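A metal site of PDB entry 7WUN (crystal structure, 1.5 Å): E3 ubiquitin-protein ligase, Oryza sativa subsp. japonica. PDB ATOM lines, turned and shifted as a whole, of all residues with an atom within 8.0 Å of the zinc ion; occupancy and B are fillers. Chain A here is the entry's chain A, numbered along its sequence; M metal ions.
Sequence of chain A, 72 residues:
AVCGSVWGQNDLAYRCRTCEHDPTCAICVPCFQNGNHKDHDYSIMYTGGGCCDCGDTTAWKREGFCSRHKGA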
ATOM      1  N   ARG A  15      18.865 -20.932 -23.582  1.00  0.00           N
ATOM      2  CA  ARG A  15      17.804 -20.276 -24.313  1.00  0.00           C
ATOM      3  C   ARG A  15      16.509 -21.003 -24.011  1.00  0.00           C
ATOM      4  O   ARG A  15      16.488 -22.222 -23.838  1.00  0.00           O
ATOM      5  CB  ARG A  15      18.046 -20.335 -25.828  1.00  0.00           C
ATOM      6  CG  ARG A  15      19.364 -19.794 -26.324  1.00  0.00           C
ATOM      7  CD  ARG A  15      19.444 -18.299 -26.218  1.00  0.00           C
ATOM      8  NE  ARG A  15      20.603 -17.793 -26.939  1.00  0.00           N
ATOM      9  CZ  ARG A  15      21.041 -16.541 -26.851  1.00  0.00           C
ATOM     10  NH1 ARG A  15      20.413 -15.646 -26.103  1.00  0.00           N
ATOM     11  NH2 ARG A  15      22.131 -16.195 -27.524  1.00  0.00           N
ATOM     12  N   CYS A  16      15.432 -20.220 -24.009  1.00  0.00           N
ATOM     13  CA  CYS A  16      14.099 -20.853 -23.966  1.00  0.00           C
ATOM     14  C   CYS A  16      13.206 -20.032 -24.900  1.00  0.00           C
ATOM     15  O   CYS A  16      12.733 -19.003 -24.469  1.00  0.00           O
ATOM     16  CB  CYS A  16      13.534 -20.976 -22.565  1.00  0.00           C
ATOM     17  SG  CYS A  16      12.006 -21.945 -22.608  1.00  0.00           S
ATOM     18  N   ARG A  17      12.837 -20.612 -26.043  1.00  0.00           N
ATOM     19  CA  ARG A  17      12.008 -19.880 -27.026  1.00  0.00           C
ATOM     20  C   ARG A  17      10.563 -19.802 -26.530  1.00  0.00           C
ATOM     21  O   ARG A  17       9.837 -18.925 -26.975  1.00  0.00           O
ATOM     22  CB  ARG A  17      12.063 -20.600 -28.373  1.00  0.00           C
ATOM     23  CG  ARG A  17      13.469 -20.900 -28.863  1.00  0.00           C
ATOM     24  CD  ARG A  17      14.333 -19.664 -28.850  1.00  0.00           C
ATOM     25  NE  ARG A  17      15.687 -19.926 -29.310  1.00  0.00           N
ATOM     26  CZ  ARG A  17      16.682 -19.048 -29.268  1.00  0.00           C
ATOM     27  NH1 ARG A  17      16.479 -17.838 -28.780  1.00  0.00           N
ATOM     28  NH2 ARG A  17      17.885 -19.392 -29.718  1.00  0.00           N
ATOM     29  N   THR A  18      10.220 -20.618 -25.530  1.00  0.00           N
ATOM     30  CA  THR A  18       8.855 -20.575 -24.949  1.00  0.00           C
ATOM     31  C   THR A  18       8.780 -19.354 -24.003  1.00  0.00           C
ATOM     32  O   THR A  18       7.751 -18.707 -23.997  1.00  0.00           O
ATOM     33  CB  THR A  18       8.542 -21.884 -24.209  1.00  0.00           C
ATOM     34  OG1 THR A  18       8.709 -22.954 -25.142  1.00  0.00           O
ATOM     35  CG2 THR A  18       7.145 -21.910 -23.631  1.00  0.00           C
ATOM     36  N   CYS A  19       9.852 -19.062 -23.288  1.00  0.00           N
ATOM     37  CA  CYS A  19       9.798 -18.021 -22.259  1.00  0.00           C
ATOM     38  C   CYS A  19      10.342 -16.673 -22.712  1.00  0.00           C
ATOM     39  O   CYS A  19      10.010 -15.653 -22.094  1.00  0.00           O
ATOM     40  CB  CYS A  19      10.587 -18.472 -21.015  1.00  0.00           C
ATOM     41  SG  CYS A  19       9.819 -19.815 -20.129  1.00  0.00           S
ATOM     42  N   GLU A  20      11.172 -16.641 -23.746  1.00  0.00           N
ATOM     43  CA  GLU A  20      11.872 -15.410 -24.106  1.00  0.00           C
ATOM     44  C   GLU A  20      10.904 -14.378 -24.678  1.00  0.00           C
ATOM     45  O   GLU A  20       9.849 -14.721 -25.222  1.00  0.00           O
ATOM     46  CB  GLU A  20      12.959 -15.702 -25.153  1.00  0.00           C
ATOM     47  CG  GLU A  20      12.372 -15.966 -26.547  1.00  0.00           C
ATOM     48  CD  GLU A  20      13.386 -16.448 -27.574  1.00  0.00           C
ATOM     49  OE1 GLU A  20      14.425 -17.035 -27.191  1.00  0.00           O
ATOM     50  OE2 GLU A  20      13.136 -16.239 -28.772  1.00  0.00           O
ATOM     51  N   ILE A  27      18.890 -17.338 -19.736  1.00  0.00           N
ATOM     52  CA  ILE A  27      19.024 -17.456 -18.280  1.00  0.00           C
ATOM     53  C   ILE A  27      20.170 -18.390 -17.930  1.00  0.00           C
ATOM     54  O   ILE A  27      20.541 -19.289 -18.699  1.00  0.00           O
ATOM     55  CB  ILE A  27      17.717 -17.909 -17.594  1.00  0.00           C
ATOM     56  CG1 ILE A  27      17.299 -19.322 -18.010  1.00  0.00           C
ATOM     57  CG2 ILE A  27      16.591 -16.904 -17.848  1.00  0.00           C
ATOM     58  CD1 ILE A  27      16.078 -19.798 -17.223  1.00  0.00           C
ATOM     59  N   PHE A  32      17.725 -21.877 -14.777  1.00  0.00           N
ATOM     60  CA  PHE A  32      16.961 -22.852 -15.549  1.00  0.00           C
ATOM     61  C   PHE A  32      16.600 -24.057 -14.688  1.00  0.00           C
ATOM     62  O   PHE A  32      15.448 -24.509 -14.673  1.00  0.00           O
ATOM     63  CB  PHE A  32      17.754 -23.312 -16.768  1.00  0.00           C
ATOM     64  CG  PHE A  32      16.985 -24.272 -17.626  1.00  0.00           C
ATOM     65  CD1 PHE A  32      16.043 -23.813 -18.540  1.00  0.00           C
ATOM     66  CD2 PHE A  32      17.132 -25.631 -17.437  1.00  0.00           C
ATOM     67  CE1 PHE A  32      15.299 -24.704 -19.315  1.00  0.00           C
ATOM     68  CE2 PHE A  32      16.378 -26.532 -18.214  1.00  0.00           C
ATOM     69  CZ  PHE A  32      15.472 -26.070 -19.131  1.00  0.00           C
ATOM     70  N   GLY A  35      13.730 -23.601 -12.293  1.00  0.00           N
ATOM     71  CA  GLY A  35      12.470 -23.200 -12.873  1.00  0.00           C
ATOM     72  C   GLY A  35      11.777 -24.367 -13.558  1.00  0.00           C
ATOM     73  O   GLY A  35      12.238 -25.512 -13.519  1.00  0.00           O
ATOM     74  N   ASN A  36      10.653 -24.056 -14.200  1.00  0.00           N
ATOM     75  CA  ASN A  36       9.765 -25.058 -14.755  1.00  0.00           C
ATOM     76  C   ASN A  36       9.674 -24.828 -16.256  1.00  0.00           C
ATOM     77  O   ASN A  36       8.995 -23.903 -16.713  1.00  0.00           O
ATOM     78  CB  ASN A  36       8.403 -24.957 -14.075  1.00  0.00           C
ATOM     79  CG  ASN A  36       8.532 -25.023 -12.551  1.00  0.00           C
ATOM     80  OD1 ASN A  36       9.243 -25.875 -12.016  1.00  0.00           O
ATOM     81  ND2 ASN A  36       7.846 -24.116 -11.855  1.00  0.00           N
ATOM     82  N   HIS A  37      10.364 -25.667 -17.027  1.00  0.00           N
ATOM     83  CA  HIS A  37      10.358 -25.539 -18.485  1.00  0.00           C
ATOM     84  C   HIS A  37      10.064 -26.862 -19.163  1.00  0.00           C
ATOM     85  O   HIS A  37      10.526 -27.119 -20.282  1.00  0.00           O
ATOM     86  CB  HIS A  37      11.685 -24.982 -18.996  1.00  0.00           C
ATOM     87  CG  HIS A  37      12.061 -23.681 -18.370  1.00  0.00           C
ATOM     88  ND1 HIS A  37      11.708 -22.471 -18.930  1.00  0.00           N
ATOM     89  CD2 HIS A  37      12.707 -23.388 -17.223  1.00  0.00           C
ATOM     90  CE1 HIS A  37      12.134 -21.491 -18.156  1.00  0.00           C
ATOM     91  NE2 HIS A  37      12.742 -22.025 -17.109  1.00  0.00           N
ATOM     92  N   LYS A  38       9.308 -27.734 -18.489  1.00  0.00           N
ATOM     93  CA  LYS A  38       8.978 -28.982 -19.144  1.00  0.00           C
ATOM     94  C   LYS A  38       8.053 -28.758 -20.331  1.00  0.00           C
ATOM     95  O   LYS A  38       7.107 -27.957 -20.285  1.00  0.00           O
ATOM     96  CB  LYS A  38       8.423 -30.010 -18.162  1.00  0.00           C
ATOM     97  CG  LYS A  38       9.382 -30.285 -17.001  1.00  0.00           C
ATOM     98  CD  LYS A  38       8.902 -31.405 -16.095  1.00  0.00           C
ATOM     99  CE  LYS A  38       9.724 -31.447 -14.823  1.00  0.00           C
ATOM    100  NZ  LYS A  38       9.237 -32.493 -13.890  1.00  0.00           N
ATOM    101  N   ASP A  39       8.400 -29.414 -21.418  1.00  0.00           N
ATOM    102  CA  ASP A  39       7.793 -29.277 -22.733  1.00  0.00           C
ATOM    103  C   ASP A  39       8.050 -27.914 -23.362  1.00  0.00           C
ATOM    104  O   ASP A  39       7.462 -27.605 -24.398  1.00  0.00           O
ATOM    105  CB  ASP A  39       6.290 -29.578 -22.700  1.00  0.00           C
ATOM    106  CG  ASP A  39       5.989 -31.053 -22.909  1.00  0.00           C
ATOM    107  OD1 ASP A  39       6.801 -31.762 -23.548  1.00  0.00           O
ATOM    108  OD2 ASP A  39       4.936 -31.510 -22.413  1.00  0.00           O
ATOM    109  N   HIS A  40       8.927 -27.098 -22.773  1.00  0.00           N
ATOM    110  CA  HIS A  40       9.340 -25.863 -23.431  1.00  0.00           C
ATOM    111  C   HIS A  40      10.367 -26.154 -24.521  1.00  0.00           C
ATOM    112  O   HIS A  40      11.051 -27.181 -24.517  1.00  0.00           O
ATOM    113  CB  HIS A  40       9.943 -24.869 -22.423  1.00  0.00           C
ATOM    114  CG  HIS A  40       8.936 -24.314 -21.464  1.00  0.00           C
ATOM    115  ND1 HIS A  40       9.161 -23.162 -20.728  1.00  0.00           N
ATOM    116  CD2 HIS A  40       7.698 -24.745 -21.126  1.00  0.00           C
ATOM    117  CE1 HIS A  40       8.105 -22.925 -19.973  1.00  0.00           C
ATOM    118  NE2 HIS A  40       7.203 -23.857 -20.202  1.00  0.00           N
ATOM    119  N   ASP A  41      10.483 -25.208 -25.442  1.00  0.00           N
ATOM    120  CA  ASP A  41      11.493 -25.268 -26.500  1.00  0.00           C
ATOM    121  C   ASP A  41      12.762 -24.615 -25.972  1.00  0.00           C
ATOM    122  O   ASP A  41      13.095 -23.479 -26.314  1.00  0.00           O
ATOM    123  CB  ASP A  41      10.989 -24.584 -27.756  1.00  0.00           C
ATOM    124  CG  ASP A  41      12.014 -24.573 -28.870  1.00  0.00           C
ATOM    125  OD1 ASP A  41      12.932 -25.412 -28.853  1.00  0.00           O
ATOM    126  OD2 ASP A  41      11.892 -23.716 -29.758  1.00  0.00           O
ATOM    127  N   TYR A  42      13.486 -25.352 -25.153  1.00  0.00           N
ATOM    128  CA  TYR A  42      14.700 -24.825 -24.554  1.00  0.00           C
ATOM    129  C   TYR A  42      15.927 -25.542 -25.092  1.00  0.00           C
ATOM    130  O   TYR A  42      15.847 -26.666 -25.592  1.00  0.00           O
ATOM    131  CB  TYR A  42      14.681 -24.956 -23.021  1.00  0.00           C
ATOM    132  CG  TYR A  42      14.682 -26.374 -22.483  1.00  0.00           C
ATOM    133  CD1 TYR A  42      15.874 -27.096 -22.339  1.00  0.00           C
ATOM    134  CD2 TYR A  42      13.500 -26.969 -22.060  1.00  0.00           C
ATOM    135  CE1 TYR A  42      15.871 -28.384 -21.841  1.00  0.00           C
ATOM    136  CE2 TYR A  42      13.493 -28.255 -21.549  1.00  0.00           C
ATOM    137  CZ  TYR A  42      14.667 -28.957 -21.452  1.00  0.00           C
ATOM    138  OH  TYR A  42      14.637 -30.238 -20.949  1.00  0.00           O
ATOM    139  N   TRP A  60      11.577 -11.898 -20.075  1.00  0.00           N
ATOM    140  CA  TRP A  60      11.305 -13.301 -19.807  1.00  0.00           C
ATOM    141  C   TRP A  60       9.906 -13.433 -19.216  1.00  0.00           C
ATOM    142  O   TRP A  60       9.495 -12.629 -18.366  1.00  0.00           O
ATOM    143  CB  TRP A  60      12.364 -13.834 -18.844  1.00  0.00           C
ATOM    144  CG  TRP A  60      12.606 -15.320 -18.854  1.00  0.00           C
ATOM    145  CD1 TRP A  60      12.123 -16.232 -17.967  1.00  0.00           C
ATOM    146  CD2 TRP A  60      13.454 -16.054 -19.757  1.00  0.00           C
ATOM    147  NE1 TRP A  60      12.581 -17.497 -18.276  1.00  0.00           N
ATOM    148  CE2 TRP A  60      13.406 -17.412 -19.371  1.00  0.00           C
ATOM    149  CE3 TRP A  60      14.230 -15.703 -20.871  1.00  0.00           C
ATOM    150  CZ2 TRP A  60      14.119 -18.408 -20.040  1.00  0.00           C
ATOM    151  CZ3 TRP A  60      14.937 -16.691 -21.543  1.00  0.00           C
ATOM    152  CH2 TRP A  60      14.877 -18.034 -21.126  1.00  0.00           C
ATOM    153  N   LYS A  61       9.162 -14.436 -19.668  1.00  0.00           N
ATOM    154  CA  LYS A  61       7.824 -14.657 -19.150  1.00  0.00           C
ATOM    155  C   LYS A  61       7.860 -15.065 -17.669  1.00  0.00           C
ATOM    156  O   LYS A  61       8.736 -15.806 -17.234  1.00  0.00           O
ATOM    157  CB  LYS A  61       7.107 -15.718 -19.993  1.00  0.00           C
ATOM    158  CG  LYS A  61       6.849 -15.217 -21.397  1.00  0.00           C
ATOM    159  CD  LYS A  61       6.102 -16.212 -22.250  1.00  0.00           C
ATOM    160  CE  LYS A  61       6.273 -15.871 -23.718  1.00  0.00           C
ATOM    161  NZ  LYS A  61       5.912 -17.003 -24.624  1.00  0.00           N
ATOM    162  N   GLU A  63       6.081 -16.994 -15.864  1.00  0.00           N
ATOM    163  CA  GLU A  63       5.987 -18.436 -15.620  1.00  0.00           C
ATOM    164  C   GLU A  63       7.343 -19.126 -15.763  1.00  0.00           C
ATOM    165  O   GLU A  63       7.509 -20.233 -15.236  1.00  0.00           O
ATOM    166  CB  GLU A  63       4.946 -19.077 -16.545  1.00  0.00           C
ATOM    167  CG  GLU A  63       3.713 -18.197 -16.851  1.00  0.00           C
ATOM    168  CD  GLU A  63       4.025 -16.962 -17.702  1.00  0.00           C
ATOM    169  OE1 GLU A  63       3.528 -15.877 -17.354  1.00  0.00           O
ATOM    170  OE2 GLU A  63       4.777 -17.070 -18.685  1.00  0.00           O
ATOM    171  N   GLY A  64       8.299 -18.505 -16.456  1.00  0.00           N
ATOM    172  CA  GLY A  64       9.633 -19.030 -16.620  1.00  0.00           C
ATOM    173  C   GLY A  64      10.661 -18.567 -15.602  1.00  0.00           C
ATOM    174  O   GLY A  64      11.830 -18.944 -15.735  1.00  0.00           O
ATOM    175  N   PHE A  65      10.265 -17.784 -14.600  1.00  0.00           N
ATOM    176  CA  PHE A  65      11.173 -17.396 -13.524  1.00  0.00           C
ATOM    177  C   PHE A  65      11.463 -18.590 -12.634  1.00  0.00           C
ATOM    178  O   PHE A  65      10.585 -19.413 -12.349  1.00  0.00           O
ATOM    179  CB  PHE A  65      10.559 -16.292 -12.662  1.00  0.00           C
ATOM    180  CG  PHE A  65      10.352 -14.980 -13.371  1.00  0.00           C
ATOM    181  CD1 PHE A  65      10.878 -14.735 -14.629  1.00  0.00           C
ATOM    182  CD2 PHE A  65       9.654 -13.960 -12.739  1.00  0.00           C
ATOM    183  CE1 PHE A  65      10.686 -13.513 -15.254  1.00  0.00           C
ATOM    184  CE2 PHE A  65       9.454 -12.723 -13.346  1.00  0.00           C
ATOM    185  CZ  PHE A  65       9.973 -12.500 -14.611  1.00  0.00           C
HETATM  186 ZN    ZN M   1      10.787 -21.854 -20.693  1.00  0.00          ZN
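O of Cys 19 is in hydrogen-bond range of N of Lys 61 (2.8 Å). N of Thr 18 sits close to SG of Cys 16, 3.7 Å away. A ring nitrogen (NE2) of His 37 lies within hydrogen-bond range of the backbone carbonyl oxygen (O) of Gly 64, 3.5 Å away.
The nearest printed residue that does not touch the zinc ion is Thr 18 (4.2 Å).
The zinc ion is bound by ND1 of His 37 (2.1 Å). A ring nitrogen (ND1) of His 40 is bound to the zinc ion (2.1 Å). SG of Cys 16 binds the zinc ion, at 2.3 Å. The zinc ion is bound by SG of Cys 19.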
